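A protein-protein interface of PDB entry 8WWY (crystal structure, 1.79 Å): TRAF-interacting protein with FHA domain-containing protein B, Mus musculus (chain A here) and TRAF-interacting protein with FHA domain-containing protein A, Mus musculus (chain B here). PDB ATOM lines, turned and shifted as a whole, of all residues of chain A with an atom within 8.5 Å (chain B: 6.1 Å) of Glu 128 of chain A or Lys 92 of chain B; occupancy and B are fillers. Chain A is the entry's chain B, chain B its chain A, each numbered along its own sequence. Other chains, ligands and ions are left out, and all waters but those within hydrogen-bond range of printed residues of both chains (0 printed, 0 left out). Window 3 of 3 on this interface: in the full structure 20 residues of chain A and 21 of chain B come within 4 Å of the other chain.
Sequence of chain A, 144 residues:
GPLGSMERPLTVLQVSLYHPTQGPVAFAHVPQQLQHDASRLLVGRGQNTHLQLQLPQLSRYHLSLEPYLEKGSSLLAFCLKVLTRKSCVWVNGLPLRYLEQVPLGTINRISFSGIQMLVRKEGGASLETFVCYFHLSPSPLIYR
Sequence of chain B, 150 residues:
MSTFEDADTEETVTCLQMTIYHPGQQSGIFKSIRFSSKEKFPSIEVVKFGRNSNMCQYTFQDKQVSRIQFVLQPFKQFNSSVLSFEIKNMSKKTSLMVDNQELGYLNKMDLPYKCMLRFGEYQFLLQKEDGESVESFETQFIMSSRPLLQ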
ATOM      1  N   PRO A   9       5.850  29.811  -3.294  1.00  0.00           N
ATOM      2  CA  PRO A   9       5.002  28.831  -3.991  1.00  0.00           C
ATOM      3  C   PRO A   9       4.222  29.416  -5.154  1.00  0.00           C
ATOM      4  O   PRO A   9       3.983  28.699  -6.128  1.00  0.00           O
ATOM      5  CB  PRO A   9       4.061  28.327  -2.888  1.00  0.00           C
ATOM      6  CG  PRO A   9       4.035  29.449  -1.886  1.00  0.00           C
ATOM      7  CD  PRO A   9       5.414  30.037  -1.905  1.00  0.00           C
ATOM      8  N   LEU A  10       3.806  30.680  -5.081  1.00  0.00           N
ATOM      9  CA  LEU A  10       3.052  31.317  -6.152  1.00  0.00           C
ATOM     10  C   LEU A  10       3.715  32.626  -6.545  1.00  0.00           C
ATOM     11  O   LEU A  10       4.245  33.348  -5.694  1.00  0.00           O
ATOM     12  CB  LEU A  10       1.587  31.638  -5.753  1.00  0.00           C
ATOM     13  CG  LEU A  10       0.686  30.652  -5.009  1.00  0.00           C
ATOM     14  CD1 LEU A  10      -0.698  31.269  -4.804  1.00  0.00           C
ATOM     15  CD2 LEU A  10       0.579  29.339  -5.744  1.00  0.00           C
ATOM     16  N   THR A  11       3.636  32.949  -7.840  1.00  0.00           N
ATOM     17  CA  THR A  11       3.875  34.322  -8.264  1.00  0.00           C
ATOM     18  C   THR A  11       2.879  35.232  -7.572  1.00  0.00           C
ATOM     19  O   THR A  11       1.685  34.923  -7.513  1.00  0.00           O
ATOM     20  CB  THR A  11       3.741  34.466  -9.788  1.00  0.00           C
ATOM     21  OG1 THR A  11       4.789  33.723 -10.424  1.00  0.00           O
ATOM     22  CG2 THR A  11       3.848  35.925 -10.196  1.00  0.00           C
ATOM     23  N   GLN A  35      -6.837  35.025  -5.398  1.00  0.00           N
ATOM     24  CA  GLN A  35      -6.052  33.936  -5.958  1.00  0.00           C
ATOM     25  C   GLN A  35      -6.719  33.480  -7.254  1.00  0.00           C
ATOM     26  O   GLN A  35      -7.885  33.072  -7.242  1.00  0.00           O
ATOM     27  CB  GLN A  35      -5.935  32.792  -4.956  1.00  0.00           C
ATOM     28  CG  GLN A  35      -5.139  31.613  -5.463  1.00  0.00           C
ATOM     29  CD  GLN A  35      -4.955  30.548  -4.401  1.00  0.00           C
ATOM     30  OE1 GLN A  35      -4.042  30.627  -3.583  1.00  0.00           O
ATOM     31  NE2 GLN A  35      -5.826  29.546  -4.407  1.00  0.00           N
ATOM     32  N   HIS A  36      -5.969  33.534  -8.352  1.00  0.00           N
ATOM     33  CA  HIS A  36      -6.484  33.334  -9.704  1.00  0.00           C
ATOM     34  C   HIS A  36      -5.855  32.092 -10.320  1.00  0.00           C
ATOM     35  O   HIS A  36      -4.843  31.583  -9.831  1.00  0.00           O
ATOM     36  CB  HIS A  36      -6.184  34.552 -10.575  1.00  0.00           C
ATOM     37  CG  HIS A  36      -7.100  34.711 -11.747  1.00  0.00           C
ATOM     38  ND1 HIS A  36      -8.371  35.235 -11.635  1.00  0.00           N
ATOM     39  CD2 HIS A  36      -6.924  34.421 -13.064  1.00  0.00           C
ATOM     40  CE1 HIS A  36      -8.933  35.280 -12.836  1.00  0.00           C
ATOM     41  NE2 HIS A  36      -8.074  34.792 -13.718  1.00  0.00           N
ATOM     42  N   ASP A  37      -6.465  31.602 -11.403  1.00  0.00           N
ATOM     43  CA  ASP A  37      -5.947  30.416 -12.083  1.00  0.00           C
ATOM     44  C   ASP A  37      -5.227  30.818 -13.363  1.00  0.00           C
ATOM     45  O   ASP A  37      -4.698  31.929 -13.455  1.00  0.00           O
ATOM     46  CB  ASP A  37      -7.067  29.406 -12.373  1.00  0.00           C
ATOM     47  CG  ASP A  37      -8.167  29.977 -13.262  1.00  0.00           C
ATOM     48  OD1 ASP A  37      -8.080  31.146 -13.677  1.00  0.00           O
ATOM     49  OD2 ASP A  37      -9.137  29.245 -13.537  1.00  0.00           O
ATOM     50  N   ALA A  38      -5.198  29.940 -14.364  1.00  0.00           N
ATOM     51  CA  ALA A  38      -4.471  30.254 -15.591  1.00  0.00           C
ATOM     52  C   ALA A  38      -5.323  30.979 -16.637  1.00  0.00           C
ATOM     53  O   ALA A  38      -4.857  31.191 -17.762  1.00  0.00           O
ATOM     54  CB  ALA A  38      -3.877  28.976 -16.185  1.00  0.00           C
ATOM     55  N   SER A  39      -6.547  31.360 -16.303  1.00  0.00           N
ATOM     56  CA  SER A  39      -7.382  32.155 -17.192  1.00  0.00           C
ATOM     57  C   SER A  39      -7.070  33.640 -17.028  1.00  0.00           C
ATOM     58  O   SER A  39      -6.403  34.060 -16.078  1.00  0.00           O
ATOM     59  CB  SER A  39      -8.865  31.884 -16.920  1.00  0.00           C
ATOM     60  OG  SER A  39      -9.256  32.343 -15.634  1.00  0.00           O
ATOM     61  N   PRO A  67      -2.088  35.307 -17.751  1.00  0.00           N
ATOM     62  CA  PRO A  67      -0.869  34.556 -17.446  1.00  0.00           C
ATOM     63  C   PRO A  67      -0.542  33.598 -18.583  1.00  0.00           C
ATOM     64  O   PRO A  67      -1.434  33.014 -19.201  1.00  0.00           O
ATOM     65  CB  PRO A  67      -1.244  33.794 -16.170  1.00  0.00           C
ATOM     66  CG  PRO A  67      -2.716  33.484 -16.377  1.00  0.00           C
ATOM     67  CD  PRO A  67      -3.277  34.707 -17.111  1.00  0.00           C
ATOM     68  N   LEU A  69       3.177  31.290 -20.480  1.00  0.00           N
ATOM     69  CA  LEU A  69       4.571  30.879 -20.387  1.00  0.00           C
ATOM     70  C   LEU A  69       5.288  31.123 -21.705  1.00  0.00           C
ATOM     71  O   LEU A  69       4.831  30.666 -22.758  1.00  0.00           O
ATOM     72  CB  LEU A  69       4.696  29.401 -20.014  1.00  0.00           C
ATOM     73  CG  LEU A  69       4.371  29.024 -18.576  1.00  0.00           C
ATOM     74  CD1 LEU A  69       4.389  27.514 -18.455  1.00  0.00           C
ATOM     75  CD2 LEU A  69       5.383  29.659 -17.608  1.00  0.00           C
ATOM     76  N   LEU A  76       5.676  32.224 -14.698  1.00  0.00           N
ATOM     77  CA  LEU A  76       4.600  32.847 -15.457  1.00  0.00           C
ATOM     78  C   LEU A  76       4.963  34.263 -15.885  1.00  0.00           C
ATOM     79  O   LEU A  76       5.541  35.042 -15.112  1.00  0.00           O
ATOM     80  CB  LEU A  76       3.318  32.896 -14.627  1.00  0.00           C
ATOM     81  CG  LEU A  76       2.644  31.560 -14.328  1.00  0.00           C
ATOM     82  CD1 LEU A  76       1.504  31.780 -13.345  1.00  0.00           C
ATOM     83  CD2 LEU A  76       2.134  30.929 -15.628  1.00  0.00           C
ATOM     84  N   GLY A 124       7.062  33.245  -8.419  1.00  0.00           N
ATOM     85  CA  GLY A 124       6.919  32.056  -7.603  1.00  0.00           C
ATOM     86  C   GLY A 124       6.780  30.828  -8.482  1.00  0.00           C
ATOM     87  O   GLY A 124       6.752  30.927  -9.707  1.00  0.00           O
ATOM     88  N   ALA A 125       6.671  29.666  -7.835  1.00  0.00           N
ATOM     89  CA  ALA A 125       6.905  28.412  -8.548  1.00  0.00           C
ATOM     90  C   ALA A 125       5.707  27.950  -9.367  1.00  0.00           C
ATOM     91  O   ALA A 125       5.894  27.321 -10.417  1.00  0.00           O
ATOM     92  CB  ALA A 125       7.312  27.307  -7.570  1.00  0.00           C
ATOM     93  N   SER A 126       4.485  28.238  -8.919  1.00  0.00           N
ATOM     94  CA  SER A 126       3.308  27.663  -9.565  1.00  0.00           C
ATOM     95  C   SER A 126       3.146  28.129 -11.008  1.00  0.00           C
ATOM     96  O   SER A 126       3.234  29.324 -11.316  1.00  0.00           O
ATOM     97  CB  SER A 126       2.033  28.019  -8.803  1.00  0.00           C
ATOM     98  OG  SER A 126       0.922  27.387  -9.428  1.00  0.00           O
ATOM     99  N   LEU A 127       2.841  27.173 -11.887  1.00  0.00           N
ATOM    100  CA  LEU A 127       2.483  27.470 -13.267  1.00  0.00           C
ATOM    101  C   LEU A 127       0.982  27.389 -13.513  1.00  0.00           C
ATOM    102  O   LEU A 127       0.551  27.471 -14.663  1.00  0.00           O
ATOM    103  CB  LEU A 127       3.228  26.522 -14.212  1.00  0.00           C
ATOM    104  CG  LEU A 127       4.735  26.448 -13.966  1.00  0.00           C
ATOM    105  CD1 LEU A 127       5.407  25.413 -14.862  1.00  0.00           C
ATOM    106  CD2 LEU A 127       5.384  27.819 -14.127  1.00  0.00           C
ATOM    107  N   GLU A 128       0.178  27.216 -12.458  1.00  0.00           N
ATOM    108  CA  GLU A 128      -1.268  27.078 -12.573  1.00  0.00           C
ATOM    109  C   GLU A 128      -2.056  28.118 -11.787  1.00  0.00           C
ATOM    110  O   GLU A 128      -3.254  28.280 -12.043  1.00  0.00           O
ATOM    111  CB  GLU A 128      -1.712  25.685 -12.090  1.00  0.00           C
ATOM    112  CG  GLU A 128      -1.068  24.524 -12.811  1.00  0.00           C
ATOM    113  CD  GLU A 128      -1.509  23.191 -12.229  1.00  0.00           C
ATOM    114  OE1 GLU A 128      -2.203  23.206 -11.189  1.00  0.00           O
ATOM    115  OE2 GLU A 128      -1.169  22.139 -12.807  1.00  0.00           O
ATOM    116  N   THR A 129      -1.415  28.843 -10.872  1.00  0.00           N
ATOM    117  CA  THR A 129      -2.091  29.702  -9.910  1.00  0.00           C
ATOM    118  C   THR A 129      -1.204  30.903  -9.608  1.00  0.00           C
ATOM    119  O   THR A 129       0.019  30.758  -9.513  1.00  0.00           O
ATOM    120  CB  THR A 129      -2.373  28.932  -8.612  1.00  0.00           C
ATOM    121  OG1 THR A 129      -3.009  27.681  -8.912  1.00  0.00           O
ATOM    122  CG2 THR A 129      -3.255  29.736  -7.684  1.00  0.00           C
ATOM    123  N   PHE A 130      -1.814  32.080  -9.431  1.00  0.00           N
ATOM    124  CA  PHE A 130      -1.079  33.240  -8.945  1.00  0.00           C
ATOM    125  C   PHE A 130      -1.992  34.005  -7.992  1.00  0.00           C
ATOM    126  O   PHE A 130      -3.200  33.753  -7.912  1.00  0.00           O
ATOM    127  CB  PHE A 130      -0.537  34.124 -10.091  1.00  0.00           C
ATOM    128  CG  PHE A 130      -1.586  34.811 -10.919  1.00  0.00           C
ATOM    129  CD1 PHE A 130      -2.226  34.143 -11.965  1.00  0.00           C
ATOM    130  CD2 PHE A 130      -1.866  36.153 -10.717  1.00  0.00           C
ATOM    131  CE1 PHE A 130      -3.172  34.796 -12.750  1.00  0.00           C
ATOM    132  CE2 PHE A 130      -2.806  36.821 -11.509  1.00  0.00           C
ATOM    133  CZ  PHE A 130      -3.464  36.144 -12.519  1.00  0.00           C
ATOM    134  N   VAL A 131      -1.412  34.908  -7.217  1.00  0.00           N
ATOM    135  CA  VAL A 131      -2.203  35.661  -6.252  1.00  0.00           C
ATOM    136  C   VAL A 131      -1.885  37.137  -6.401  1.00  0.00           C
ATOM    137  O   VAL A 131      -0.728  37.517  -6.618  1.00  0.00           O
ATOM    138  CB  VAL A 131      -1.966  35.176  -4.804  1.00  0.00           C
ATOM    139  CG1 VAL A 131      -0.491  35.246  -4.418  1.00  0.00           C
ATOM    140  CG2 VAL A 131      -2.819  35.972  -3.829  1.00  0.00           C
ATOM    141  N   SER B  66      -8.752  17.550 -23.296  1.00  0.00           N
ATOM    142  CA  SER B  66      -8.680  18.211 -21.996  1.00  0.00           C
ATOM    143  C   SER B  66      -9.913  19.083 -21.791  1.00  0.00           C
ATOM    144  O   SER B  66     -10.579  19.491 -22.745  1.00  0.00           O
ATOM    145  CB  SER B  66      -7.418  19.069 -21.886  1.00  0.00           C
ATOM    146  OG  SER B  66      -6.247  18.292 -22.069  1.00  0.00           O
ATOM    147  N   ASN B  89      -2.032  27.061 -25.915  1.00  0.00           N
ATOM    148  CA  ASN B  89      -2.338  25.721 -25.446  1.00  0.00           C
ATOM    149  C   ASN B  89      -2.667  25.770 -23.956  1.00  0.00           C
ATOM    150  O   ASN B  89      -1.890  26.310 -23.161  1.00  0.00           O
ATOM    151  CB  ASN B  89      -1.153  24.794 -25.717  1.00  0.00           C
ATOM    152  CG  ASN B  89      -1.455  23.358 -25.382  1.00  0.00           C
ATOM    153  OD1 ASN B  89      -2.590  23.020 -25.062  1.00  0.00           O
ATOM    154  ND2 ASN B  89      -0.443  22.488 -25.489  1.00  0.00           N
ATOM    155  N   MET B  90      -3.829  25.227 -23.578  1.00  0.00           N
ATOM    156  CA  MET B  90      -4.223  25.165 -22.167  1.00  0.00           C
ATOM    157  C   MET B  90      -4.044  23.782 -21.566  1.00  0.00           C
ATOM    158  O   MET B  90      -4.321  23.601 -20.374  1.00  0.00           O
ATOM    159  CB  MET B  90      -5.690  25.589 -21.973  1.00  0.00           C
ATOM    160  CG  MET B  90      -6.038  26.981 -22.440  1.00  0.00           C
ATOM    161  SD  MET B  90      -5.113  28.273 -21.590  1.00  0.00           S
ATOM    162  CE  MET B  90      -5.634  28.008 -19.897  1.00  0.00           C
ATOM    163  N   SER B  91      -3.603  22.803 -22.351  1.00  0.00           N
ATOM    164  CA  SER B  91      -3.522  21.425 -21.888  1.00  0.00           C
ATOM    165  C   SER B  91      -2.176  21.162 -21.226  1.00  0.00           C
ATOM    166  O   SER B  91      -1.124  21.469 -21.793  1.00  0.00           O
ATOM    167  CB  SER B  91      -3.731  20.453 -23.051  1.00  0.00           C
ATOM    168  OG  SER B  91      -3.595  19.106 -22.630  1.00  0.00           O
ATOM    169  N   LYS B  92      -2.214  20.568 -20.032  1.00  0.00           N
ATOM    170  CA  LYS B  92      -0.982  20.138 -19.388  1.00  0.00           C
ATOM    171  C   LYS B  92      -0.400  18.885 -20.020  1.00  0.00           C
ATOM    172  O   LYS B  92       0.800  18.635 -19.875  1.00  0.00           O
ATOM    173  CB  LYS B  92      -1.230  19.883 -17.901  1.00  0.00           C
ATOM    174  CG  LYS B  92      -1.786  21.084 -17.175  1.00  0.00           C
ATOM    175  CD  LYS B  92      -1.097  21.253 -15.835  1.00  0.00           C
ATOM    176  CE  LYS B  92       0.406  21.403 -16.023  1.00  0.00           C
ATOM    177  NZ  LYS B  92       1.124  21.641 -14.740  1.00  0.00           N
ATOM    178  N   LYS B  93      -1.216  18.090 -20.707  1.00  0.00           N
ATOM    179  CA  LYS B  93      -0.785  16.774 -21.156  1.00  0.00           C
ATOM    180  C   LYS B  93      -0.544  16.672 -22.653  1.00  0.00           C
ATOM    181  O   LYS B  93       0.252  15.829 -23.077  1.00  0.00           O
ATOM    182  CB  LYS B  93      -1.817  15.715 -20.745  1.00  0.00           C
ATOM    183  CG  LYS B  93      -2.084  15.691 -19.247  1.00  0.00           C
ATOM    184  CD  LYS B  93      -2.778  14.409 -18.810  1.00  0.00           C
ATOM    185  CE  LYS B  93      -2.843  14.308 -17.291  1.00  0.00           C
ATOM    186  NZ  LYS B  93      -3.436  13.017 -16.833  1.00  0.00           N
ATOM    187  N   THR B  94      -1.197  17.496 -23.465  1.00  0.00           N
ATOM    188  CA  THR B  94      -1.208  17.316 -24.915  1.00  0.00           C
ATOM    189  C   THR B  94      -0.609  18.542 -25.585  1.00  0.00           C
ATOM    190  O   THR B  94      -1.149  19.643 -25.462  1.00  0.00           O
ATOM    191  CB  THR B  94      -2.633  17.088 -25.418  1.00  0.00           C
ATOM    192  OG1 THR B  94      -3.211  15.982 -24.715  1.00  0.00           O
ATOM    193  CG2 THR B  94      -2.643  16.805 -26.919  1.00  0.00           C
ATOM    194  N   TYR B 105       2.297  23.606 -22.558  1.00  0.00           N
ATOM    195  CA  TYR B 105       1.308  24.178 -21.652  1.00  0.00           C
ATOM    196  C   TYR B 105       1.529  25.675 -21.468  1.00  0.00           C
ATOM    197  O   TYR B 105       2.622  26.114 -21.108  1.00  0.00           O
ATOM    198  CB  TYR B 105       1.367  23.456 -20.308  1.00  0.00           C
ATOM    199  CG  TYR B 105       0.613  24.154 -19.203  1.00  0.00           C
ATOM    200  CD1 TYR B 105      -0.778  24.184 -19.190  1.00  0.00           C
ATOM    201  CD2 TYR B 105       1.298  24.780 -18.163  1.00  0.00           C
ATOM    202  CE1 TYR B 105      -1.472  24.829 -18.160  1.00  0.00           C
ATOM    203  CE2 TYR B 105       0.613  25.418 -17.136  1.00  0.00           C
ATOM    204  CZ  TYR B 105      -0.771  25.441 -17.146  1.00  0.00           C
ATOM    205  OH  TYR B 105      -1.448  26.089 -16.129  1.00  0.00           O
ATOM    206  N   LEU B 106       0.479  26.453 -21.724  1.00  0.00           N
ATOM    207  CA  LEU B 106       0.443  27.914 -21.633  1.00  0.00           C
ATOM    208  C   LEU B 106       1.386  28.617 -22.609  1.00  0.00           C
ATOM    209  O   LEU B 106       1.604  29.825 -22.474  1.00  0.00           O
ATOM    210  CB  LEU B 106       0.718  28.408 -20.203  1.00  0.00           C
ATOM    211  CG  LEU B 106      -0.369  28.155 -19.161  1.00  0.00           C
ATOM    212  CD1 LEU B 106       0.013  28.845 -17.830  1.00  0.00           C
ATOM    213  CD2 LEU B 106      -1.725  28.627 -19.638  1.00  0.00           C
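O of Leu 106 of chain B lies within hydrogen-bond range of N of Leu 69 of chain A. OE2 of Glu 128 of chain A is in salt-bridge range of NZ of Lys 92 of chain B (3.0 Å). The backbone carbonyl oxygen (O) of Leu 127 of chain A sits at hydrogen-bond distance from the side-chain hydroxyl (OH) of Tyr 105 of chain B (2.8 Å).
Glu 128 of chain A touches just these residues of chain B: Lys 92 (3.0 Å) and Tyr 105 (3.7 Å). Of the printed residues of chain A, Lys 92 of chain B touches Glu 128. No residue of chain A comes within 4 Å of Ser 91 of chain B. Of the printed residues of chain B, Leu 76 of chain A touches Leu 106 (3.7 Å). Of the printed residues of chain A, Leu 106 of chain B touches Leu 69, Leu 76 and Leu 127. Gly 124 of chain A touches none of the printed residues of chain B. Val 131 of chain A touches none of the printed residues of chain B. The nearest residue of chain B that does not touch Glu 128 of chain A is Leu 106 of chain B (5.6 Å). The nearest printed residue of chain A that does not touch Tyr 105 of chain B is Leu 76 of chain A (5.9 Å).
Among the printed residues, pairs that only touch across the chains: Leu 69 of chain A with Tyr 105 of chain B, Leu 127 of chain A with Leu 106 of chain B, Glu 128 of chain A with Tyr 105 of chain B, Leu 76 of chain A with Leu 106 of chain B, Ala 38 of chain A with Tyr 105 of chain B and Ala 38 of chain A with Met 90 of chain B.
Hydrophobic or aromatic side chains of chain A that line the printed part of chain B: Ala 38, Leu 69 and Leu 76.
The backbone carbonyl oxygen (O) of Asn 89 of chain B lies within hydrogen-bond range of the backbone NH (N) of Leu 106 of chain B (2.8 Å). OG of Ser 126 of chain A sits at hydrogen-bond distance from N of Glu 128 of chain A (3.1 Å). N of Ala 38 of chain A lies within hydrogen-bond range of O of Glu 128 of chain A.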
